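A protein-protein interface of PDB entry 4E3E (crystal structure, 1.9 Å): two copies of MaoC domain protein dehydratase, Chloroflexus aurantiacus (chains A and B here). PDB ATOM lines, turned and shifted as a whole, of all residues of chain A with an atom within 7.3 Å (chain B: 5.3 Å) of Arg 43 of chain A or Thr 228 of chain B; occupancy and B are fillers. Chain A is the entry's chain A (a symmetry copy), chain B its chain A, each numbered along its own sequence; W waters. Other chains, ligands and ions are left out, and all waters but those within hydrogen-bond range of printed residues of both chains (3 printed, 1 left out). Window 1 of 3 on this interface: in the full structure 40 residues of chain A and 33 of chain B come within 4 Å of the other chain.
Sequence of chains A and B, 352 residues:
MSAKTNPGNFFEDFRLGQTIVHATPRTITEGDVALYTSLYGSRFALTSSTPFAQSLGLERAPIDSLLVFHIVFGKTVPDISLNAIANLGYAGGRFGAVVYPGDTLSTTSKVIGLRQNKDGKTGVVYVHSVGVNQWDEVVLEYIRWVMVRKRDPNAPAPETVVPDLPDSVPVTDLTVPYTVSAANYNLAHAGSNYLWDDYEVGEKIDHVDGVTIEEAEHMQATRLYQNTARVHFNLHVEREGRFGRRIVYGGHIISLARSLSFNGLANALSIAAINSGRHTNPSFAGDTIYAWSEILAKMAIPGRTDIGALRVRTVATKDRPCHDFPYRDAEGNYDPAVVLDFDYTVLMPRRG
The side-chain hydroxyl (OG) of Ser 48 of chain A lies within hydrogen-bond range of the side-chain amide nitrogen (NE2) of Gln 226 of chain B. The guanidinium group (NE) of Arg 230 of chain B lies within salt-bridge range of the side-chain carboxylate (OD2) of Asp 209 of chain A. The backbone NH (N) of Thr 24 of chain B lies within hydrogen-bond range of the backbone carbonyl oxygen (O) of His 189 of chain A (2.8 Å). O of Ser 42 of chain A lies within hydrogen-bond range of NE2 of Gln 226 of chain B (2.9 Å).
The side-chain carboxylate (OD1) of Asp 209 of chain A is in hydrogen-bond range of the side-chain amide nitrogen (ND2) of Asn 263 of chain A (3.4 Å). N of Ser 42 of chain A lies within hydrogen-bond range of OG of Ser 259 of chain A (3.4 Å).
Among the printed residues, pairs that only touch across the chains: Arg 43 of chain A with Thr 228 of chain B (3.3 Å), Arg 43 of chain A with Thr 24 of chain B (3.3 Å), Arg 43 of chain A with Pro 78 of chain B (3.4 Å), Val 211 of chain A with Phe 233 of chain B (3.8 Å), Arg 43 of chain A with Gln 226 of chain B (3.9 Å) and Asn 263 of chain A with Arg 230 of chain B (3.9 Å).
Arg 43 of chain A touches four residues of chain B. Of chain A, only Arg 43 comes within 4 Å of Thr 228 of chain B. Printed residues of chain B within 4 Å of Asp 209 of chain A: Arg 230 (2.8 Å). Of the printed residues of chain B, Ser 42 of chain A touches Gln 226. Of the printed residues of chain A, Pro 78 of chain B touches Arg 43. Of the printed residues of chain A, Arg 230 of chain B touches Asp 209 and Asn 263. Of the printed residues of chain A, Thr 24 of chain B touches Arg 43 (3.3 Å) and His 189 (2.8 Å). The nearest residue of chain A that does not touch Thr 228 of chain B is Asp 209 of chain A (4.2 Å). The nearest printed residue of chain B that does not touch His 189 of chain A is Gln 226 of chain B (9.3 Å).
Of the 21 printed residues of chain A, 7 touch a printed residue of chain B. Hydrophobic or aromatic side chains of chain A that line the printed part of chain B: Val 211. Printed residues of chain B that touch a printed residue of chain A: Thr 24, Pro 78, Gln 226, Thr 228, Arg 230 and Phe 233. Hydrophobic or aromatic side chains of chain B within 4 Å of the printed part of chain A: Pro 78 and Phe 233. Among the printed residues, 10 pairs touch across the chains.
No position is printed for both chains. Of the 10 pairs that touch across the chains among the printed residues, none has its exchanged pair printed and touching as well.
Water W3 bridges the side-chain carboxylate (OD2) of Asp 209 of chain A (2.7 Å) and the backbone carbonyl oxygen (O) of Thr 228 of chain B (2.8 Å). Water W2 lies within hydrogen-bond range of the side-chain hydroxyl of Thr 228 of chain B and the guanidinium group of Arg 43 of chain A. Water W1 lies within hydrogen-bond range of the guanidinium group of Arg 230 of chain B and the side-chain amide nitrogen of Asn 263 of chain A.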
ATOM      1  N   THR A  37     -28.119  22.394  -0.939  1.00  0.00           N
ATOM      2  CA  THR A  37     -27.420  21.904   0.266  1.00  0.00           C
ATOM      3  C   THR A  37     -26.927  20.447   0.099  1.00  0.00           C
ATOM      4  O   THR A  37     -25.794  20.130   0.465  1.00  0.00           O
ATOM      5  CB  THR A  37     -28.289  22.019   1.497  1.00  0.00           C
ATOM      6  OG1 THR A  37     -28.665  23.389   1.637  1.00  0.00           O
ATOM      7  CG2 THR A  37     -27.551  21.538   2.766  1.00  0.00           C
ATOM      8  N   TYR A  40     -23.881  20.251  -2.464  1.00  0.00           N
ATOM      9  CA  TYR A  40     -22.572  20.855  -2.159  1.00  0.00           C
ATOM     10  C   TYR A  40     -22.169  20.823  -0.686  1.00  0.00           C
ATOM     11  O   TYR A  40     -20.994  20.982  -0.368  1.00  0.00           O
ATOM     12  CB  TYR A  40     -22.452  22.271  -2.740  1.00  0.00           C
ATOM     13  CG  TYR A  40     -22.743  22.307  -4.226  1.00  0.00           C
ATOM     14  CD1 TYR A  40     -21.774  21.916  -5.154  1.00  0.00           C
ATOM     15  CD2 TYR A  40     -24.000  22.685  -4.703  1.00  0.00           C
ATOM     16  CE1 TYR A  40     -22.033  21.932  -6.512  1.00  0.00           C
ATOM     17  CE2 TYR A  40     -24.276  22.696  -6.069  1.00  0.00           C
ATOM     18  CZ  TYR A  40     -23.285  22.324  -6.967  1.00  0.00           C
ATOM     19  OH  TYR A  40     -23.542  22.322  -8.322  1.00  0.00           O
ATOM     20  N   GLY A  41     -23.134  20.619   0.208  1.00  0.00           N
ATOM     21  CA  GLY A  41     -22.844  20.573   1.638  1.00  0.00           C
ATOM     22  C   GLY A  41     -22.459  21.922   2.234  1.00  0.00           C
ATOM     23  O   GLY A  41     -21.765  21.968   3.239  1.00  0.00           O
ATOM     24  N   SER A  42     -22.915  23.027   1.640  1.00  0.00           N
ATOM     25  CA  SER A  42     -22.497  24.327   2.133  1.00  0.00           C
ATOM     26  C   SER A  42     -22.987  24.541   3.575  1.00  0.00           C
ATOM     27  O   SER A  42     -24.160  24.316   3.888  1.00  0.00           O
ATOM     28  CB  SER A  42     -22.971  25.457   1.221  1.00  0.00           C
ATOM     29  OG  SER A  42     -22.999  26.687   1.926  1.00  0.00           O
ATOM     30  N   ARG A  43     -22.074  24.954   4.450  1.00  0.00           N
ATOM     31  CA  ARG A  43     -22.425  25.169   5.860  1.00  0.00           C
ATOM     32  C   ARG A  43     -22.561  26.635   6.267  1.00  0.00           C
ATOM     33  O   ARG A  43     -22.725  26.918   7.449  1.00  0.00           O
ATOM     34  CB  ARG A  43     -21.433  24.462   6.783  1.00  0.00           C
ATOM     35  CG  ARG A  43     -21.589  22.950   6.801  1.00  0.00           C
ATOM     36  CD  ARG A  43     -20.791  22.372   7.951  1.00  0.00           C
ATOM     37  NE  ARG A  43     -19.383  22.274   7.584  1.00  0.00           N
ATOM     38  CZ  ARG A  43     -18.369  22.435   8.429  1.00  0.00           C
ATOM     39  NH1 ARG A  43     -18.604  22.713   9.705  1.00  0.00           N
ATOM     40  NH2 ARG A  43     -17.121  22.324   7.990  1.00  0.00           N
ATOM     41  N   PHE A  44     -22.498  27.564   5.306  1.00  0.00           N
ATOM     42  CA  PHE A  44     -22.609  28.993   5.630  1.00  0.00           C
ATOM     43  C   PHE A  44     -23.914  29.286   6.341  1.00  0.00           C
ATOM     44  O   PHE A  44     -24.989  28.884   5.879  1.00  0.00           O
ATOM     45  CB  PHE A  44     -22.418  29.871   4.387  1.00  0.00           C
ATOM     46  CG  PHE A  44     -20.999  29.864   3.895  1.00  0.00           C
ATOM     47  CD1 PHE A  44     -20.044  30.687   4.494  1.00  0.00           C
ATOM     48  CD2 PHE A  44     -20.592  28.963   2.908  1.00  0.00           C
ATOM     49  CE1 PHE A  44     -18.716  30.650   4.081  1.00  0.00           C
ATOM     50  CE2 PHE A  44     -19.267  28.924   2.487  1.00  0.00           C
ATOM     51  CZ  PHE A  44     -18.323  29.768   3.075  1.00  0.00           C
ATOM     52  N   ALA A  45     -23.811  29.954   7.484  1.00  0.00           N
ATOM     53  CA  ALA A  45     -24.962  30.058   8.396  1.00  0.00           C
ATOM     54  C   ALA A  45     -26.116  30.870   7.834  1.00  0.00           C
ATOM     55  O   ALA A  45     -27.294  30.584   8.124  1.00  0.00           O
ATOM     56  CB  ALA A  45     -24.535  30.584   9.764  1.00  0.00           C
ATOM     57  N   LEU A  46     -25.778  31.870   7.026  1.00  0.00           N
ATOM     58  CA  LEU A  46     -26.778  32.765   6.414  1.00  0.00           C
ATOM     59  C   LEU A  46     -27.844  31.984   5.611  1.00  0.00           C
ATOM     60  O   LEU A  46     -29.028  32.278   5.714  1.00  0.00           O
ATOM     61  CB  LEU A  46     -26.093  33.819   5.512  1.00  0.00           C
ATOM     62  CG  LEU A  46     -27.023  34.886   4.914  1.00  0.00           C
ATOM     63  CD1 LEU A  46     -27.715  35.650   6.038  1.00  0.00           C
ATOM     64  CD2 LEU A  46     -26.281  35.823   3.970  1.00  0.00           C
ATOM     65  N   THR A  47     -27.417  30.982   4.831  1.00  0.00           N
ATOM     66  CA  THR A  47     -28.363  30.273   3.977  1.00  0.00           C
ATOM     67  C   THR A  47     -29.053  29.100   4.703  1.00  0.00           C
ATOM     68  O   THR A  47     -30.121  28.672   4.283  1.00  0.00           O
ATOM     69  CB  THR A  47     -27.692  29.776   2.699  1.00  0.00           C
ATOM     70  OG1 THR A  47     -26.505  29.084   3.068  1.00  0.00           O
ATOM     71  CG2 THR A  47     -27.317  30.968   1.761  1.00  0.00           C
ATOM     72  N   SER A  48     -28.461  28.605   5.799  1.00  0.00           N
ATOM     73  CA  SER A  48     -28.982  27.415   6.511  1.00  0.00           C
ATOM     74  C   SER A  48     -30.034  27.703   7.559  1.00  0.00           C
ATOM     75  O   SER A  48     -30.817  26.823   7.900  1.00  0.00           O
ATOM     76  CB  SER A  48     -27.860  26.629   7.170  1.00  0.00           C
ATOM     77  OG  SER A  48     -27.168  25.879   6.187  1.00  0.00           O
ATOM     78  N   HIS A 189     -22.307  29.841  16.233  1.00  0.00           N
ATOM     79  CA  HIS A 189     -23.228  29.428  15.169  1.00  0.00           C
ATOM     80  C   HIS A 189     -22.648  29.675  13.797  1.00  0.00           C
ATOM     81  O   HIS A 189     -22.812  28.842  12.910  1.00  0.00           O
ATOM     82  CB  HIS A 189     -24.586  30.125  15.320  1.00  0.00           C
ATOM     83  CG  HIS A 189     -25.468  29.520  16.392  1.00  0.00           C
ATOM     84  ND1 HIS A 189     -26.720  29.966  16.638  1.00  0.00           N
ATOM     85  CD2 HIS A 189     -25.253  28.449  17.265  1.00  0.00           C
ATOM     86  CE1 HIS A 189     -27.270  29.236  17.630  1.00  0.00           C
ATOM     87  NE2 HIS A 189     -26.372  28.307  18.013  1.00  0.00           N
ATOM     88  N   ALA A 190     -21.958  30.807  13.600  1.00  0.00           N
ATOM     89  CA  ALA A 190     -21.375  31.104  12.300  1.00  0.00           C
ATOM     90  C   ALA A 190     -20.278  30.092  11.967  1.00  0.00           C
ATOM     91  O   ALA A 190     -20.160  29.660  10.830  1.00  0.00           O
ATOM     92  CB  ALA A 190     -20.831  32.515  12.253  1.00  0.00           C
ATOM     93  N   GLY A 191     -19.485  29.721  12.969  1.00  0.00           N
ATOM     94  CA  GLY A 191     -18.480  28.691  12.794  1.00  0.00           C
ATOM     95  C   GLY A 191     -17.038  29.157  12.881  1.00  0.00           C
ATOM     96  O   GLY A 191     -16.125  28.365  12.667  1.00  0.00           O
ATOM     97  N   ASP A 209     -10.191  19.820   3.021  1.00  0.00           N
ATOM     98  CA  ASP A 209     -11.079  18.739   2.576  1.00  0.00           C
ATOM     99  C   ASP A 209     -11.057  18.505   1.056  1.00  0.00           C
ATOM    100  O   ASP A 209     -10.934  19.443   0.263  1.00  0.00           O
ATOM    101  CB  ASP A 209     -12.527  18.997   3.026  1.00  0.00           C
ATOM    102  CG  ASP A 209     -12.661  19.138   4.538  1.00  0.00           C
ATOM    103  OD1 ASP A 209     -12.275  20.194   5.100  1.00  0.00           O
ATOM    104  OD2 ASP A 209     -13.181  18.196   5.169  1.00  0.00           O
ATOM    105  N   VAL A 211     -13.411  16.404  -2.025  1.00  0.00           N
ATOM    106  CA  VAL A 211     -14.689  15.733  -2.308  1.00  0.00           C
ATOM    107  C   VAL A 211     -14.730  15.180  -3.726  1.00  0.00           C
ATOM    108  O   VAL A 211     -14.353  15.865  -4.695  1.00  0.00           O
ATOM    109  CB  VAL A 211     -15.928  16.631  -2.037  1.00  0.00           C
ATOM    110  CG1 VAL A 211     -15.999  16.995  -0.560  1.00  0.00           C
ATOM    111  CG2 VAL A 211     -15.946  17.883  -2.921  1.00  0.00           C
ATOM    112  N   ARG A 258     -16.599  26.900  -3.140  1.00  0.00           N
ATOM    113  CA  ARG A 258     -17.194  27.790  -2.162  1.00  0.00           C
ATOM    114  C   ARG A 258     -17.565  27.008  -0.895  1.00  0.00           C
ATOM    115  O   ARG A 258     -17.272  27.455   0.231  1.00  0.00           O
ATOM    116  CB  ARG A 258     -18.402  28.513  -2.770  1.00  0.00           C
ATOM    117  CG  ARG A 258     -19.315  29.256  -1.784  1.00  0.00           C
ATOM    118  CD  ARG A 258     -18.704  30.457  -1.055  1.00  0.00           C
ATOM    119  NE  ARG A 258     -19.785  31.167  -0.344  1.00  0.00           N
ATOM    120  CZ  ARG A 258     -19.625  32.037   0.648  1.00  0.00           C
ATOM    121  NH1 ARG A 258     -18.401  32.370   1.089  1.00  0.00           N
ATOM    122  NH2 ARG A 258     -20.702  32.593   1.196  1.00  0.00           N
ATOM    123  N   SER A 259     -18.194  25.840  -1.073  1.00  0.00           N
ATOM    124  CA  SER A 259     -18.554  25.008   0.063  1.00  0.00           C
ATOM    125  C   SER A 259     -17.314  24.627   0.883  1.00  0.00           C
ATOM    126  O   SER A 259     -17.290  24.827   2.091  1.00  0.00           O
ATOM    127  CB  SER A 259     -19.299  23.762  -0.397  1.00  0.00           C
ATOM    128  OG  SER A 259     -19.677  23.024   0.743  1.00  0.00           O
ATOM    129  N   LEU A 260     -16.279  24.110   0.221  1.00  0.00           N
ATOM    130  CA  LEU A 260     -15.026  23.765   0.886  1.00  0.00           C
ATOM    131  C   LEU A 260     -14.371  24.950   1.600  1.00  0.00           C
ATOM    132  O   LEU A 260     -13.755  24.786   2.665  1.00  0.00           O
ATOM    133  CB  LEU A 260     -14.032  23.231  -0.146  1.00  0.00           C
ATOM    134  CG  LEU A 260     -14.349  21.914  -0.845  1.00  0.00           C
ATOM    135  CD1 LEU A 260     -13.359  21.682  -1.975  1.00  0.00           C
ATOM    136  CD2 LEU A 260     -14.356  20.749   0.139  1.00  0.00           C
ATOM    137  N   PHE A 262     -15.645  27.094   3.355  1.00  0.00           N
ATOM    138  CA  PHE A 262     -16.197  27.239   4.724  1.00  0.00           C
ATOM    139  C   PHE A 262     -15.139  26.918   5.783  1.00  0.00           C
ATOM    140  O   PHE A 262     -15.102  27.545   6.841  1.00  0.00           O
ATOM    141  CB  PHE A 262     -17.429  26.358   4.972  1.00  0.00           C
ATOM    142  CG  PHE A 262     -18.066  26.574   6.356  1.00  0.00           C
ATOM    143  CD1 PHE A 262     -18.976  27.604   6.571  1.00  0.00           C
ATOM    144  CD2 PHE A 262     -17.724  25.758   7.432  1.00  0.00           C
ATOM    145  CE1 PHE A 262     -19.540  27.814   7.822  1.00  0.00           C
ATOM    146  CE2 PHE A 262     -18.278  25.957   8.691  1.00  0.00           C
ATOM    147  CZ  PHE A 262     -19.194  26.987   8.888  1.00  0.00           C
ATOM    148  N   ASN A 263     -14.293  25.927   5.499  1.00  0.00           N
ATOM    149  CA  ASN A 263     -13.174  25.619   6.356  1.00  0.00           C
ATOM    150  C   ASN A 263     -12.095  26.674   6.142  1.00  0.00           C
ATOM    151  O   ASN A 263     -11.183  26.483   5.330  1.00  0.00           O
ATOM    152  CB  ASN A 263     -12.618  24.204   6.068  1.00  0.00           C
ATOM    153  CG  ASN A 263     -11.606  23.766   7.110  1.00  0.00           C
ATOM    154  OD1 ASN A 263     -11.542  24.342   8.197  1.00  0.00           O
ATOM    155  ND2 ASN A 263     -10.804  22.746   6.790  1.00  0.00           N
ATOM    156  N   ALA A 266     -15.380  30.854   7.126  1.00  0.00           N
ATOM    157  CA  ALA A 266     -16.747  30.668   7.633  1.00  0.00           C
ATOM    158  C   ALA A 266     -17.554  31.969   7.768  1.00  0.00           C
ATOM    159  O   ALA A 266     -18.765  31.965   7.547  1.00  0.00           O
ATOM    160  CB  ALA A 266     -16.727  29.918   8.961  1.00  0.00           C
ATOM    161  N   THR B  24     -23.624  26.204  12.602  1.00  0.00           N
ATOM    162  CA  THR B  24     -24.594  25.872  11.598  1.00  0.00           C
ATOM    163  C   THR B  24     -25.931  25.372  12.028  1.00  0.00           C
ATOM    164  O   THR B  24     -26.315  24.296  11.725  1.00  0.00           O
ATOM    165  CB  THR B  24     -24.019  24.816  10.641  1.00  0.00           C
ATOM    166  OG1 THR B  24     -22.639  25.022  10.517  1.00  0.00           O
ATOM    167  CG2 THR B  24     -24.646  24.911   9.315  1.00  0.00           C
ATOM    168  N   GLY B  74     -25.076  15.346  12.677  1.00  0.00           N
ATOM    169  CA  GLY B  74     -24.206  16.020  11.708  1.00  0.00           C
ATOM    170  C   GLY B  74     -23.551  17.297  12.224  1.00  0.00           C
ATOM    171  O   GLY B  74     -22.372  17.523  11.981  1.00  0.00           O
ATOM    172  N   VAL B  77     -20.422  16.655  14.251  1.00  0.00           N
ATOM    173  CA  VAL B  77     -19.281  15.996  13.576  1.00  0.00           C
ATOM    174  C   VAL B  77     -17.984  16.845  13.488  1.00  0.00           C
ATOM    175  O   VAL B  77     -16.894  16.342  13.834  1.00  0.00           O
ATOM    176  CB  VAL B  77     -19.691  15.397  12.215  1.00  0.00           C
ATOM    177  CG1 VAL B  77     -18.467  14.906  11.427  1.00  0.00           C
ATOM    178  CG2 VAL B  77     -20.676  14.249  12.433  1.00  0.00           C
ATOM    179  N   PRO B  78     -18.081  18.124  13.046  1.00  0.00           N
ATOM    180  CA  PRO B  78     -16.852  18.938  12.958  1.00  0.00           C
ATOM    181  C   PRO B  78     -16.042  18.980  14.268  1.00  0.00           C
ATOM    182  O   PRO B  78     -14.814  18.906  14.225  1.00  0.00           O
ATOM    183  CB  PRO B  78     -17.387  20.341  12.609  1.00  0.00           C
ATOM    184  CG  PRO B  78     -18.685  20.078  11.913  1.00  0.00           C
ATOM    185  CD  PRO B  78     -19.277  18.924  12.687  1.00  0.00           C
ATOM    186  N   LEU B  82     -14.689  14.513  13.716  1.00  0.00           N
ATOM    187  CA  LEU B  82     -13.846  14.787  12.554  1.00  0.00           C
ATOM    188  C   LEU B  82     -12.585  13.897  12.553  1.00  0.00           C
ATOM    189  O   LEU B  82     -12.206  13.355  11.519  1.00  0.00           O
ATOM    190  CB  LEU B  82     -13.477  16.273  12.461  1.00  0.00           C
ATOM    191  CG  LEU B  82     -12.812  16.702  11.142  1.00  0.00           C
ATOM    192  CD1 LEU B  82     -13.717  16.442   9.941  1.00  0.00           C
ATOM    193  CD2 LEU B  82     -12.389  18.166  11.183  1.00  0.00           C
ATOM    194  N   THR B 222     -25.522  12.483   3.338  1.00  0.00           N
ATOM    195  CA  THR B 222     -24.520  13.019   4.286  1.00  0.00           C
ATOM    196  C   THR B 222     -24.389  14.557   4.184  1.00  0.00           C
ATOM    197  O   THR B 222     -24.251  15.249   5.215  1.00  0.00           O
ATOM    198  CB  THR B 222     -23.168  12.296   4.106  1.00  0.00           C
ATOM    199  OG1 THR B 222     -23.402  10.875   4.126  1.00  0.00           O
ATOM    200  CG2 THR B 222     -22.169  12.660   5.227  1.00  0.00           C
ATOM    201  N   GLN B 226     -25.275  18.005   6.531  1.00  0.00           N
ATOM    202  CA  GLN B 226     -24.109  18.897   6.726  1.00  0.00           C
ATOM    203  C   GLN B 226     -23.075  18.191   7.646  1.00  0.00           C
ATOM    204  O   GLN B 226     -22.475  18.770   8.558  1.00  0.00           O
ATOM    205  CB  GLN B 226     -24.573  20.282   7.199  1.00  0.00           C
ATOM    206  CG  GLN B 226     -25.287  21.066   6.081  1.00  0.00           C
ATOM    207  CD  GLN B 226     -26.097  22.216   6.639  1.00  0.00           C
ATOM    208  OE1 GLN B 226     -26.847  22.028   7.587  1.00  0.00           O
ATOM    209  NE2 GLN B 226     -25.923  23.423   6.077  1.00  0.00           N
ATOM    210  N   ASN B 227     -22.927  16.898   7.386  1.00  0.00           N
ATOM    211  CA  ASN B 227     -21.996  16.017   8.087  1.00  0.00           C
ATOM    212  C   ASN B 227     -20.749  15.991   7.214  1.00  0.00           C
ATOM    213  O   ASN B 227     -20.825  15.687   6.030  1.00  0.00           O
ATOM    214  CB  ASN B 227     -22.644  14.623   8.254  1.00  0.00           C
ATOM    215  CG  ASN B 227     -21.679  13.537   8.772  1.00  0.00           C
ATOM    216  OD1 ASN B 227     -20.469  13.602   8.589  1.00  0.00           O
ATOM    217  ND2 ASN B 227     -22.242  12.517   9.422  1.00  0.00           N
ATOM    218  N   THR B 228     -19.606  16.350   7.791  1.00  0.00           N
ATOM    219  CA  THR B 228     -18.399  16.573   6.997  1.00  0.00           C
ATOM    220  C   THR B 228     -17.340  15.489   7.088  1.00  0.00           C
ATOM    221  O   THR B 228     -16.250  15.717   6.576  1.00  0.00           O
ATOM    222  CB  THR B 228     -17.666  17.853   7.424  1.00  0.00           C
ATOM    223  OG1 THR B 228     -17.279  17.724   8.803  1.00  0.00           O
ATOM    224  CG2 THR B 228     -18.569  19.090   7.268  1.00  0.00           C
ATOM    225  N   ALA B 229     -17.612  14.369   7.771  1.00  0.00           N
ATOM    226  CA  ALA B 229     -16.567  13.356   8.001  1.00  0.00           C
ATOM    227  C   ALA B 229     -15.996  12.929   6.663  1.00  0.00           C
ATOM    228  O   ALA B 229     -16.735  12.654   5.730  1.00  0.00           O
ATOM    229  CB  ALA B 229     -17.090  12.147   8.802  1.00  0.00           C
ATOM    230  N   ARG B 230     -14.676  12.867   6.593  1.00  0.00           N
ATOM    231  CA  ARG B 230     -13.943  12.807   5.321  1.00  0.00           C
ATOM    232  C   ARG B 230     -13.908  11.419   4.671  1.00  0.00           C
ATOM    233  O   ARG B 230     -13.751  11.303   3.441  1.00  0.00           O
ATOM    234  CB  ARG B 230     -12.531  13.386   5.516  1.00  0.00           C
ATOM    235  CG  ARG B 230     -12.540  14.869   5.894  1.00  0.00           C
ATOM    236  CD  ARG B 230     -11.304  15.370   6.643  1.00  0.00           C
ATOM    237  NE  ARG B 230     -11.416  16.826   6.796  1.00  0.00           N
ATOM    238  CZ  ARG B 230     -10.652  17.605   7.561  1.00  0.00           C
ATOM    239  NH1 ARG B 230      -9.659  17.098   8.287  1.00  0.00           N
ATOM    240  NH2 ARG B 230     -10.890  18.913   7.592  1.00  0.00           N
ATOM    241  N   PHE B 233     -16.405  11.047   1.744  1.00  0.00           N
ATOM    242  CA  PHE B 233     -16.381  11.923   0.566  1.00  0.00           C
ATOM    243  C   PHE B 233     -15.209  11.774  -0.380  1.00  0.00           C
ATOM    244  O   PHE B 233     -15.348  12.038  -1.579  1.00  0.00           O
ATOM    245  CB  PHE B 233     -16.469  13.389   1.001  1.00  0.00           C
ATOM    246  CG  PHE B 233     -17.777  13.748   1.648  1.00  0.00           C
ATOM    247  CD1 PHE B 233     -18.918  13.924   0.882  1.00  0.00           C
ATOM    248  CD2 PHE B 233     -17.864  13.901   3.025  1.00  0.00           C
ATOM    249  CE1 PHE B 233     -20.132  14.255   1.478  1.00  0.00           C
ATOM    250  CE2 PHE B 233     -19.069  14.234   3.635  1.00  0.00           C
ATOM    251  CZ  PHE B 233     -20.207  14.410   2.857  1.00  0.00           C
HETATM  252  O   HOH W   1      -9.412  21.113   8.896  1.00  0.00           O
HETATM  253  O   HOH W   2     -15.560  19.798   9.524  1.00  0.00           O
HETATM  254  O   HOH W   3     -15.318  16.792   4.165  1.00  0.00           O
